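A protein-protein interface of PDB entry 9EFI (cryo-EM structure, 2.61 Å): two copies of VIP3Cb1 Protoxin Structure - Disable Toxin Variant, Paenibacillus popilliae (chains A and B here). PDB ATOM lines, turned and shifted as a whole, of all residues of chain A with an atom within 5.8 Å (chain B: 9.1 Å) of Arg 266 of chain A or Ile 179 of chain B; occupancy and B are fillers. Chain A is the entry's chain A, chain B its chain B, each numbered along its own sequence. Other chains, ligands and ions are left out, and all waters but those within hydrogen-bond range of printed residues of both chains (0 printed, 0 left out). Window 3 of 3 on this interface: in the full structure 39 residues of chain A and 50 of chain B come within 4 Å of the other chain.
Of the 17 printed residues of chain A, 4 touch a printed residue of chain B.
Of the 19 printed residues of chain B, 5 touch a printed residue of chain A.
Hydrophobic or aromatic side chains of chain B that line the printed part of chain A: Ile 179.
Among the printed residues, no Asp or Glu carboxylate lies within 4 Å of a Lys or Arg side-chain nitrogen of the other chain.
Among the printed residues, pairs that only touch across the chains: Thr 184 of chain A with Thr 184 of chain B, Glu 185 of chain A with Thr 184 of chain B, Glu 185 of chain A with Thr 187 of chain B, Phe 264 of chain A with Thr 182 of chain B and Arg 266 of chain A with Ile 179 of chain B.
Thr 184 of chain B touches its own counterpart, Thr 184 of chain A.
Glu 185 of chain A touches Thr 184 of chain B, but with the chains exchanged Thr 184 of chain A does not touch Glu 185 of chain B (7.5 Å).
7 positions are printed for both chains.
Of the 7 pairs that touch across the chains among the printed residues, 1 has its exchanged pair printed and touching as well.
No residue of chain B comes within 4 Å of Cys 181 of chain A.
Of the printed residues of chain B, Thr 184 of chain A touches Thr 184.
Printed residues of chain B within 4 Å of Glu 185 of chain A: Thr 184 and Thr 187.
Gly 260 of chain A touches none of the printed residues of chain B.
No residue of chain B comes within 4 Å of Gly 265 of chain A.
Of chain B, only Ile 179 and Thr 182 come within 4 Å of Arg 266 of chain A.
No residue of chain B comes within 4 Å of Ser 267 of chain A.
Ala 268 of chain A touches none of the printed residues of chain B.
Of chain A, only Arg 266 comes within 4 Å of Ile 179 of chain B.
Printed residues of chain A within 4 Å of Cys 183 of chain B: Phe 264.
Printed residues of chain A within 4 Å of Thr 184 of chain B: Thr 184 (3.8 Å) and Glu 185 (3.6 Å).
Printed residues of chain A within 4 Å of Thr 187 of chain B: Glu 185 (3.5 Å).
The nearest residue of chain B that does not touch Arg 266 of chain A is Leu 178 of chain B (4.04 Å).
The backbone NH (N) of Cys 183 of chain B sits at hydrogen-bond distance from the backbone carbonyl oxygen (O) of Phe 264 of chain A (3.3 Å).
NH1 of Arg 266 of chain A lies within hydrogen-bond range of OG1 of Thr 182 of chain B, at 2.5 Å.
O of Cys 183 of chain B sits at hydrogen-bond distance from OG1 of Thr 187 of chain B (3.5 Å).
SG of Cys 181 of chain A is in hydrogen-bond range of NH2 of Arg 266 of chain A.
The side-chain amide oxygen of Asn 262 of chain A sits close to the backbone NH of Phe 264 of chain A (3.4 Å).
The side-chain sulfur (SG) of Cys 183 of chain B lies close to the backbone NH (N) of Glu 185 of chain B, 3.7 Å away.
The backbone carbonyl oxygen of Ile 179 of chain B is in hydrogen-bond range of the side-chain hydroxyl of Thr 182 of chain B, 2.6 Å away.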
ATOM      1  N   LEU A 178      15.145  -9.274   0.911  1.00  0.00           N
ATOM      2  CA  LEU A 178      14.693  -9.933  -0.310  1.00  0.00           C
ATOM      3  C   LEU A 178      14.291 -11.382  -0.059  1.00  0.00           C
ATOM      4  O   LEU A 178      13.300 -11.858  -0.624  1.00  0.00           O
ATOM      5  CB  LEU A 178      15.776  -9.863  -1.385  1.00  0.00           C
ATOM      6  CG  LEU A 178      15.870  -8.547  -2.158  1.00  0.00           C
ATOM      7  CD1 LEU A 178      16.838  -8.686  -3.318  1.00  0.00           C
ATOM      8  CD2 LEU A 178      14.497  -8.120  -2.653  1.00  0.00           C
ATOM      9  N   ASN A 180      12.962 -12.655   2.443  1.00  0.00           N
ATOM     10  CA  ASN A 180      11.638 -12.671   3.050  1.00  0.00           C
ATOM     11  C   ASN A 180      10.570 -12.104   2.127  1.00  0.00           C
ATOM     12  O   ASN A 180       9.403 -12.034   2.523  1.00  0.00           O
ATOM     13  CB  ASN A 180      11.647 -11.896   4.371  1.00  0.00           C
ATOM     14  CG  ASN A 180      12.360 -12.644   5.480  1.00  0.00           C
ATOM     15  OD1 ASN A 180      13.110 -13.587   5.226  1.00  0.00           O
ATOM     16  ND2 ASN A 180      12.127 -12.228   6.719  1.00  0.00           N
ATOM     17  N   CYS A 181      10.944 -11.686   0.920  1.00  0.00           N
ATOM     18  CA  CYS A 181       9.985 -11.272  -0.095  1.00  0.00           C
ATOM     19  C   CYS A 181       9.676 -12.368  -1.101  1.00  0.00           C
ATOM     20  O   CYS A 181       8.561 -12.413  -1.628  1.00  0.00           O
ATOM     21  CB  CYS A 181      10.497 -10.036  -0.843  1.00  0.00           C
ATOM     22  SG  CYS A 181      10.403  -8.497   0.101  1.00  0.00           S
ATOM     23  N   THR A 182      10.637 -13.249  -1.380  1.00  0.00           N
ATOM     24  CA  THR A 182      10.394 -14.362  -2.297  1.00  0.00           C
ATOM     25  C   THR A 182       9.757 -15.542  -1.564  1.00  0.00           C
ATOM     26  O   THR A 182       8.754 -16.101  -2.017  1.00  0.00           O
ATOM     27  CB  THR A 182      11.701 -14.774  -2.986  1.00  0.00           C
ATOM     28  OG1 THR A 182      11.548 -16.072  -3.574  1.00  0.00           O
ATOM     29  CG2 THR A 182      12.861 -14.792  -1.999  1.00  0.00           C
ATOM     30  N   THR A 184       7.856 -15.909   1.043  1.00  0.00           N
ATOM     31  CA  THR A 184       6.820 -15.503   1.985  1.00  0.00           C
ATOM     32  C   THR A 184       5.446 -15.883   1.449  1.00  0.00           C
ATOM     33  O   THR A 184       4.506 -16.096   2.221  1.00  0.00           O
ATOM     34  CB  THR A 184       6.891 -14.001   2.266  1.00  0.00           C
ATOM     35  OG1 THR A 184       5.828 -13.629   3.152  1.00  0.00           O
ATOM     36  CG2 THR A 184       6.774 -13.203   0.976  1.00  0.00           C
ATOM     37  N   GLU A 185       5.323 -15.967   0.126  1.00  0.00           N
ATOM     38  CA  GLU A 185       4.103 -16.427  -0.519  1.00  0.00           C
ATOM     39  C   GLU A 185       4.245 -17.801  -1.147  1.00  0.00           C
ATOM     40  O   GLU A 185       3.268 -18.552  -1.192  1.00  0.00           O
ATOM     41  CB  GLU A 185       3.663 -15.430  -1.600  1.00  0.00           C
ATOM     42  CG  GLU A 185       3.518 -14.005  -1.100  1.00  0.00           C
ATOM     43  CD  GLU A 185       3.133 -13.038  -2.200  1.00  0.00           C
ATOM     44  OE1 GLU A 185       2.919 -13.491  -3.344  1.00  0.00           O
ATOM     45  OE2 GLU A 185       3.043 -11.823  -1.921  1.00  0.00           O
ATOM     46  N   VAL A 257       2.059 -17.647  -7.756  1.00  0.00           N
ATOM     47  CA  VAL A 257       3.077 -16.866  -7.065  1.00  0.00           C
ATOM     48  C   VAL A 257       4.334 -16.750  -7.917  1.00  0.00           C
ATOM     49  O   VAL A 257       4.983 -15.698  -7.946  1.00  0.00           O
ATOM     50  CB  VAL A 257       3.374 -17.479  -5.684  1.00  0.00           C
ATOM     51  CG1 VAL A 257       4.560 -16.790  -5.034  1.00  0.00           C
ATOM     52  CG2 VAL A 257       2.151 -17.374  -4.792  1.00  0.00           C
ATOM     53  N   LEU A 258       4.698 -17.820  -8.632  1.00  0.00           N
ATOM     54  CA  LEU A 258       5.867 -17.746  -9.503  1.00  0.00           C
ATOM     55  C   LEU A 258       5.671 -16.715 -10.608  1.00  0.00           C
ATOM     56  O   LEU A 258       6.590 -15.951 -10.923  1.00  0.00           O
ATOM     57  CB  LEU A 258       6.174 -19.116 -10.103  1.00  0.00           C
ATOM     58  CG  LEU A 258       6.748 -20.164  -9.153  1.00  0.00           C
ATOM     59  CD1 LEU A 258       7.419 -21.275  -9.939  1.00  0.00           C
ATOM     60  CD2 LEU A 258       7.720 -19.524  -8.178  1.00  0.00           C
ATOM     61  N   ILE A 259       4.483 -16.679 -11.210  1.00  0.00           N
ATOM     62  CA  ILE A 259       4.232 -15.735 -12.293  1.00  0.00           C
ATOM     63  C   ILE A 259       3.860 -14.365 -11.745  1.00  0.00           C
ATOM     64  O   ILE A 259       4.350 -13.338 -12.226  1.00  0.00           O
ATOM     65  CB  ILE A 259       3.141 -16.282 -13.231  1.00  0.00           C
ATOM     66  CG1 ILE A 259       3.516 -17.676 -13.723  1.00  0.00           C
ATOM     67  CG2 ILE A 259       2.940 -15.346 -14.410  1.00  0.00           C
ATOM     68  CD1 ILE A 259       4.818 -17.715 -14.467  1.00  0.00           C
ATOM     69  N   GLY A 260       2.990 -14.323 -10.740  1.00  0.00           N
ATOM     70  CA  GLY A 260       2.513 -13.063 -10.208  1.00  0.00           C
ATOM     71  C   GLY A 260       1.268 -12.572 -10.916  1.00  0.00           C
ATOM     72  O   GLY A 260       1.191 -11.405 -11.310  1.00  0.00           O
ATOM     73  N   ASN A 262      -1.798 -12.165  -9.679  1.00  0.00           N
ATOM     74  CA  ASN A 262      -2.512 -11.195  -8.866  1.00  0.00           C
ATOM     75  C   ASN A 262      -1.761  -9.870  -8.829  1.00  0.00           C
ATOM     76  O   ASN A 262      -0.528  -9.825  -8.855  1.00  0.00           O
ATOM     77  CB  ASN A 262      -2.713 -11.725  -7.446  1.00  0.00           C
ATOM     78  CG  ASN A 262      -1.423 -11.777  -6.654  1.00  0.00           C
ATOM     79  OD1 ASN A 262      -1.267 -11.071  -5.657  1.00  0.00           O
ATOM     80  ND2 ASN A 262      -0.493 -12.618  -7.089  1.00  0.00           N
ATOM     81  N   PHE A 264      -1.776  -7.759  -6.335  1.00  0.00           N
ATOM     82  CA  PHE A 264      -1.235  -7.480  -5.009  1.00  0.00           C
ATOM     83  C   PHE A 264       0.185  -8.013  -4.867  1.00  0.00           C
ATOM     84  O   PHE A 264       1.085  -7.298  -4.413  1.00  0.00           O
ATOM     85  CB  PHE A 264      -2.135  -8.088  -3.933  1.00  0.00           C
ATOM     86  CG  PHE A 264      -3.588  -7.754  -4.094  1.00  0.00           C
ATOM     87  CD1 PHE A 264      -4.096  -6.564  -3.605  1.00  0.00           C
ATOM     88  CD2 PHE A 264      -4.448  -8.639  -4.720  1.00  0.00           C
ATOM     89  CE1 PHE A 264      -5.434  -6.259  -3.746  1.00  0.00           C
ATOM     90  CE2 PHE A 264      -5.786  -8.339  -4.864  1.00  0.00           C
ATOM     91  CZ  PHE A 264      -6.280  -7.149  -4.374  1.00  0.00           C
ATOM     92  N   GLY A 265       0.403  -9.269  -5.252  1.00  0.00           N
ATOM     93  CA  GLY A 265       1.682  -9.912  -5.050  1.00  0.00           C
ATOM     94  C   GLY A 265       2.692  -9.587  -6.131  1.00  0.00           C
ATOM     95  O   GLY A 265       2.415  -8.910  -7.120  1.00  0.00           O
ATOM     96  N   ARG A 266       3.903 -10.094  -5.922  1.00  0.00           N
ATOM     97  CA  ARG A 266       5.011  -9.926  -6.847  1.00  0.00           C
ATOM     98  C   ARG A 266       5.479 -11.290  -7.334  1.00  0.00           C
ATOM     99  O   ARG A 266       5.349 -12.294  -6.629  1.00  0.00           O
ATOM    100  CB  ARG A 266       6.172  -9.175  -6.186  1.00  0.00           C
ATOM    101  CG  ARG A 266       6.536  -9.707  -4.810  1.00  0.00           C
ATOM    102  CD  ARG A 266       7.552  -8.819  -4.116  1.00  0.00           C
ATOM    103  NE  ARG A 266       7.761  -9.220  -2.729  1.00  0.00           N
ATOM    104  CZ  ARG A 266       7.035  -8.786  -1.708  1.00  0.00           C
ATOM    105  NH1 ARG A 266       6.044  -7.927  -1.880  1.00  0.00           N
ATOM    106  NH2 ARG A 266       7.309  -9.225  -0.483  1.00  0.00           N
ATOM    107  N   SER A 267       6.016 -11.317  -8.551  1.00  0.00           N
ATOM    108  CA  SER A 267       6.487 -12.568  -9.130  1.00  0.00           C
ATOM    109  C   SER A 267       7.633 -13.131  -8.304  1.00  0.00           C
ATOM    110  O   SER A 267       8.638 -12.450  -8.075  1.00  0.00           O
ATOM    111  CB  SER A 267       6.930 -12.343 -10.574  1.00  0.00           C
ATOM    112  OG  SER A 267       7.424 -13.543 -11.144  1.00  0.00           O
ATOM    113  N   ALA A 268       7.479 -14.379  -7.855  1.00  0.00           N
ATOM    114  CA  ALA A 268       8.518 -15.002  -7.042  1.00  0.00           C
ATOM    115  C   ALA A 268       9.785 -15.244  -7.853  1.00  0.00           C
ATOM    116  O   ALA A 268      10.896 -15.133  -7.323  1.00  0.00           O
ATOM    117  CB  ALA A 268       8.005 -16.308  -6.441  1.00  0.00           C
ATOM    118  N   THR A 271      11.814 -11.792  -8.114  1.00  0.00           N
ATOM    119  CA  THR A 271      12.482 -11.399  -6.878  1.00  0.00           C
ATOM    120  C   THR A 271      13.559 -12.401  -6.478  1.00  0.00           C
ATOM    121  O   THR A 271      14.594 -12.006  -5.930  1.00  0.00           O
ATOM    122  CB  THR A 271      11.468 -11.215  -5.748  1.00  0.00           C
ATOM    123  OG1 THR A 271      12.161 -10.943  -4.522  1.00  0.00           O
ATOM    124  CG2 THR A 271      10.618 -12.453  -5.572  1.00  0.00           C
ATOM    125  N   ASP B 171       4.758  -5.682 -14.870  1.00  0.00           N
ATOM    126  CA  ASP B 171       5.892  -6.584 -14.695  1.00  0.00           C
ATOM    127  C   ASP B 171       6.985  -6.361 -15.730  1.00  0.00           C
ATOM    128  O   ASP B 171       8.142  -6.711 -15.472  1.00  0.00           O
ATOM    129  CB  ASP B 171       5.424  -8.040 -14.740  1.00  0.00           C
ATOM    130  CG  ASP B 171       4.878  -8.435 -16.095  1.00  0.00           C
ATOM    131  OD1 ASP B 171       4.281  -7.572 -16.768  1.00  0.00           O
ATOM    132  OD2 ASP B 171       5.047  -9.609 -16.487  1.00  0.00           O
ATOM    133  N   ASN B 174       9.489  -2.458 -14.199  1.00  0.00           N
ATOM    134  CA  ASN B 174       9.428  -2.182 -12.770  1.00  0.00           C
ATOM    135  C   ASN B 174      10.740  -2.616 -12.134  1.00  0.00           C
ATOM    136  O   ASN B 174      11.610  -3.197 -12.787  1.00  0.00           O
ATOM    137  CB  ASN B 174       8.237  -2.882 -12.106  1.00  0.00           C
ATOM    138  CG  ASN B 174       7.048  -1.958 -11.925  1.00  0.00           C
ATOM    139  OD1 ASN B 174       6.883  -1.338 -10.875  1.00  0.00           O
ATOM    140  ND2 ASN B 174       6.216  -1.857 -12.954  1.00  0.00           N
ATOM    141  N   LEU B 175      10.866  -2.325 -10.845  1.00  0.00           N
ATOM    142  CA  LEU B 175      12.081  -2.614 -10.093  1.00  0.00           C
ATOM    143  C   LEU B 175      11.682  -2.896  -8.648  1.00  0.00           C
ATOM    144  O   LEU B 175      10.514  -3.175  -8.358  1.00  0.00           O
ATOM    145  CB  LEU B 175      13.092  -1.460 -10.229  1.00  0.00           C
ATOM    146  CG  LEU B 175      12.746  -0.087  -9.641  1.00  0.00           C
ATOM    147  CD1 LEU B 175      14.019   0.696  -9.363  1.00  0.00           C
ATOM    148  CD2 LEU B 175      11.835   0.705 -10.567  1.00  0.00           C
ATOM    149  N   ASN B 176      12.657  -2.827  -7.737  1.00  0.00           N
ATOM    150  CA  ASN B 176      12.391  -3.099  -6.328  1.00  0.00           C
ATOM    151  C   ASN B 176      11.423  -2.098  -5.712  1.00  0.00           C
ATOM    152  O   ASN B 176      10.890  -2.357  -4.628  1.00  0.00           O
ATOM    153  CB  ASN B 176      13.703  -3.107  -5.542  1.00  0.00           C
ATOM    154  CG  ASN B 176      14.428  -1.778  -5.607  1.00  0.00           C
ATOM    155  OD1 ASN B 176      15.197  -1.522  -6.533  1.00  0.00           O
ATOM    156  ND2 ASN B 176      14.187  -0.922  -4.620  1.00  0.00           N
ATOM    157  N   VAL B 177      11.190  -0.960  -6.372  1.00  0.00           N
ATOM    158  CA  VAL B 177      10.206   0.001  -5.882  1.00  0.00           C
ATOM    159  C   VAL B 177       8.823  -0.637  -5.831  1.00  0.00           C
ATOM    160  O   VAL B 177       8.031  -0.372  -4.917  1.00  0.00           O
ATOM    161  CB  VAL B 177      10.217   1.271  -6.754  1.00  0.00           C
ATOM    162  CG1 VAL B 177       9.174   2.265  -6.267  1.00  0.00           C
ATOM    163  CG2 VAL B 177      11.600   1.903  -6.747  1.00  0.00           C
ATOM    164  N   LEU B 178       8.513  -1.494  -6.810  1.00  0.00           N
ATOM    165  CA  LEU B 178       7.254  -2.230  -6.789  1.00  0.00           C
ATOM    166  C   LEU B 178       7.114  -3.062  -5.520  1.00  0.00           C
ATOM    167  O   LEU B 178       5.992  -3.308  -5.063  1.00  0.00           O
ATOM    168  CB  LEU B 178       7.149  -3.119  -8.032  1.00  0.00           C
ATOM    169  CG  LEU B 178       5.923  -4.023  -8.187  1.00  0.00           C
ATOM    170  CD1 LEU B 178       5.437  -4.019  -9.625  1.00  0.00           C
ATOM    171  CD2 LEU B 178       6.238  -5.445  -7.744  1.00  0.00           C
ATOM    172  N   ILE B 179       8.235  -3.493  -4.936  1.00  0.00           N
ATOM    173  CA  ILE B 179       8.189  -4.230  -3.676  1.00  0.00           C
ATOM    174  C   ILE B 179       7.527  -3.388  -2.594  1.00  0.00           C
ATOM    175  O   ILE B 179       6.740  -3.894  -1.784  1.00  0.00           O
ATOM    176  CB  ILE B 179       9.607  -4.678  -3.268  1.00  0.00           C
ATOM    177  CG1 ILE B 179       9.954  -6.033  -3.896  1.00  0.00           C
ATOM    178  CG2 ILE B 179       9.748  -4.744  -1.753  1.00  0.00           C
ATOM    179  CD1 ILE B 179      10.193  -5.992  -5.392  1.00  0.00           C
ATOM    180  N   ASN B 180       7.816  -2.084  -2.576  1.00  0.00           N
ATOM    181  CA  ASN B 180       7.196  -1.185  -1.612  1.00  0.00           C
ATOM    182  C   ASN B 180       5.710  -0.973  -1.869  1.00  0.00           C
ATOM    183  O   ASN B 180       5.027  -0.408  -1.008  1.00  0.00           O
ATOM    184  CB  ASN B 180       7.916   0.165  -1.619  1.00  0.00           C
ATOM    185  CG  ASN B 180       9.402   0.034  -1.347  1.00  0.00           C
ATOM    186  OD1 ASN B 180       9.838  -0.882  -0.650  1.00  0.00           O
ATOM    187  ND2 ASN B 180      10.186   0.952  -1.897  1.00  0.00           N
ATOM    188  N   CYS B 181       5.196  -1.407  -3.018  1.00  0.00           N
ATOM    189  CA  CYS B 181       3.795  -1.235  -3.380  1.00  0.00           C
ATOM    190  C   CYS B 181       3.114  -2.582  -3.592  1.00  0.00           C
ATOM    191  O   CYS B 181       2.355  -2.774  -4.544  1.00  0.00           O
ATOM    192  CB  CYS B 181       3.660  -0.363  -4.626  1.00  0.00           C
ATOM    193  SG  CYS B 181       4.354   1.297  -4.453  1.00  0.00           S
ATOM    194  N   THR B 182       3.382  -3.534  -2.702  1.00  0.00           N
ATOM    195  CA  THR B 182       2.782  -4.858  -2.767  1.00  0.00           C
ATOM    196  C   THR B 182       2.251  -5.251  -1.397  1.00  0.00           C
ATOM    197  O   THR B 182       2.808  -4.869  -0.363  1.00  0.00           O
ATOM    198  CB  THR B 182       3.782  -5.917  -3.252  1.00  0.00           C
ATOM    199  OG1 THR B 182       5.026  -5.758  -2.557  1.00  0.00           O
ATOM    200  CG2 THR B 182       4.014  -5.791  -4.750  1.00  0.00           C
ATOM    201  N   CYS B 183       1.168  -6.023  -1.400  1.00  0.00           N
ATOM    202  CA  CYS B 183       0.531  -6.499  -0.182  1.00  0.00           C
ATOM    203  C   CYS B 183       0.613  -8.016  -0.130  1.00  0.00           C
ATOM    204  O   CYS B 183       0.273  -8.694  -1.106  1.00  0.00           O
ATOM    205  CB  CYS B 183      -0.929  -6.043  -0.106  1.00  0.00           C
ATOM    206  SG  CYS B 183      -1.790  -6.552   1.399  1.00  0.00           S
ATOM    207  N   THR B 184       1.062  -8.543   1.009  1.00  0.00           N
ATOM    208  CA  THR B 184       1.158  -9.979   1.220  1.00  0.00           C
ATOM    209  C   THR B 184       0.061 -10.526   2.121  1.00  0.00           C
ATOM    210  O   THR B 184      -0.272 -11.710   2.015  1.00  0.00           O
ATOM    211  CB  THR B 184       2.527 -10.333   1.822  1.00  0.00           C
ATOM    212  OG1 THR B 184       3.556  -9.634   1.110  1.00  0.00           O
ATOM    213  CG2 THR B 184       2.795 -11.827   1.729  1.00  0.00           C
ATOM    214  N   GLU B 185      -0.519  -9.689   2.982  1.00  0.00           N
ATOM    215  CA  GLU B 185      -1.570 -10.134   3.888  1.00  0.00           C
ATOM    216  C   GLU B 185      -2.824 -10.587   3.151  1.00  0.00           C
ATOM    217  O   GLU B 185      -3.601 -11.377   3.699  1.00  0.00           O
ATOM    218  CB  GLU B 185      -1.910  -9.006   4.866  1.00  0.00           C
ATOM    219  CG  GLU B 185      -2.853  -9.393   5.986  1.00  0.00           C
ATOM    220  CD  GLU B 185      -3.153  -8.237   6.918  1.00  0.00           C
ATOM    221  OE1 GLU B 185      -2.606  -7.137   6.695  1.00  0.00           O
ATOM    222  OE2 GLU B 185      -3.935  -8.428   7.872  1.00  0.00           O
ATOM    223  N   THR B 187      -2.819 -12.008  -0.064  1.00  0.00           N
ATOM    224  CA  THR B 187      -2.579 -13.058  -1.053  1.00  0.00           C
ATOM    225  C   THR B 187      -3.266 -14.377  -0.713  1.00  0.00           C
ATOM    226  O   THR B 187      -3.901 -14.958  -1.611  1.00  0.00           O
ATOM    227  CB  THR B 187      -1.069 -13.248  -1.243  1.00  0.00           C
ATOM    228  OG1 THR B 187      -0.488 -12.022  -1.704  1.00  0.00           O
ATOM    229  CG2 THR B 187      -0.793 -14.343  -2.259  1.00  0.00           C
ATOM    230  N   GLN B 191      -6.156 -15.764  -3.260  1.00  0.00           N
ATOM    231  CA  GLN B 191      -5.926 -17.013  -3.978  1.00  0.00           C
ATOM    232  C   GLN B 191      -7.006 -18.035  -3.653  1.00  0.00           C
ATOM    233  O   GLN B 191      -7.507 -18.724  -4.550  1.00  0.00           O
ATOM    234  CB  GLN B 191      -4.543 -17.571  -3.641  1.00  0.00           C
ATOM    235  CG  GLN B 191      -3.382 -16.751  -4.179  1.00  0.00           C
ATOM    236  CD  GLN B 191      -3.285 -16.788  -5.692  1.00  0.00           C
ATOM    237  OE1 GLN B 191      -2.792 -15.848  -6.315  1.00  0.00           O
ATOM    238  NE2 GLN B 191      -3.746 -17.881  -6.289  1.00  0.00           N
ATOM    239  N   THR B 271      -3.081   0.702  -1.533  1.00  0.00           N
ATOM    240  CA  THR B 271      -1.790   0.264  -2.054  1.00  0.00           C
ATOM    241  C   THR B 271      -1.887  -0.097  -3.530  1.00  0.00           C
ATOM    242  O   THR B 271      -1.033   0.295  -4.334  1.00  0.00           O
ATOM    243  CB  THR B 271      -1.272  -0.926  -1.245  1.00  0.00           C
ATOM    244  OG1 THR B 271      -1.145  -0.552   0.132  1.00  0.00           O
ATOM    245  CG2 THR B 271       0.082  -1.376  -1.767  1.00  0.00           C
ATOM    246  N   GLU B 274      -2.274   3.178  -5.587  1.00  0.00           N
ATOM    247  CA  GLU B 274      -1.012   3.884  -5.776  1.00  0.00           C
ATOM    248  C   GLU B 274      -0.042   3.094  -6.645  1.00  0.00           C
ATOM    249  O   GLU B 274       0.850   3.692  -7.254  1.00  0.00           O
ATOM    250  CB  GLU B 274      -0.372   4.210  -4.424  1.00  0.00           C
ATOM    251  CG  GLU B 274       0.306   3.037  -3.743  1.00  0.00           C
ATOM    252  CD  GLU B 274       0.922   3.415  -2.411  1.00  0.00           C
ATOM    253  OE1 GLU B 274       0.711   4.561  -1.962  1.00  0.00           O
ATOM    254  OE2 GLU B 274       1.617   2.568  -1.813  1.00  0.00           O
ATOM    255  N   LEU B 275      -0.195   1.770  -6.714  1.00  0.00           N
ATOM    256  CA  LEU B 275       0.606   0.988  -7.649  1.00  0.00           C
ATOM    257  C   LEU B 275       0.140   1.199  -9.086  1.00  0.00           C
ATOM    258  O   LEU B 275       0.965   1.311 -10.001  1.00  0.00           O
ATOM    259  CB  LEU B 275       0.546  -0.492  -7.277  1.00  0.00           C
ATOM    260  CG  LEU B 275       1.223  -1.465  -8.243  1.00  0.00           C
ATOM    261  CD1 LEU B 275       2.710  -1.171  -8.342  1.00  0.00           C
ATOM    262  CD2 LEU B 275       0.982  -2.904  -7.813  1.00  0.00           C
ATOM    263  N   LYS B 278       0.954   4.699 -11.157  1.00  0.00           N
ATOM    264  CA  LYS B 278       2.299   5.047 -11.591  1.00  0.00           C
ATOM    265  C   LYS B 278       2.298   5.411 -13.070  1.00  0.00           C
ATOM    266  O   LYS B 278       1.630   4.769 -13.886  1.00  0.00           O
ATOM    267  CB  LYS B 278       3.259   3.889 -11.330  1.00  0.00           C
ATOM    268  CG  LYS B 278       3.444   3.559  -9.859  1.00  0.00           C
ATOM    269  CD  LYS B 278       4.447   2.435  -9.667  1.00  0.00           C
ATOM    270  CE  LYS B 278       4.647   2.123  -8.195  1.00  0.00           C
ATOM    271  NZ  LYS B 278       5.123   3.312  -7.437  1.00  0.00           N
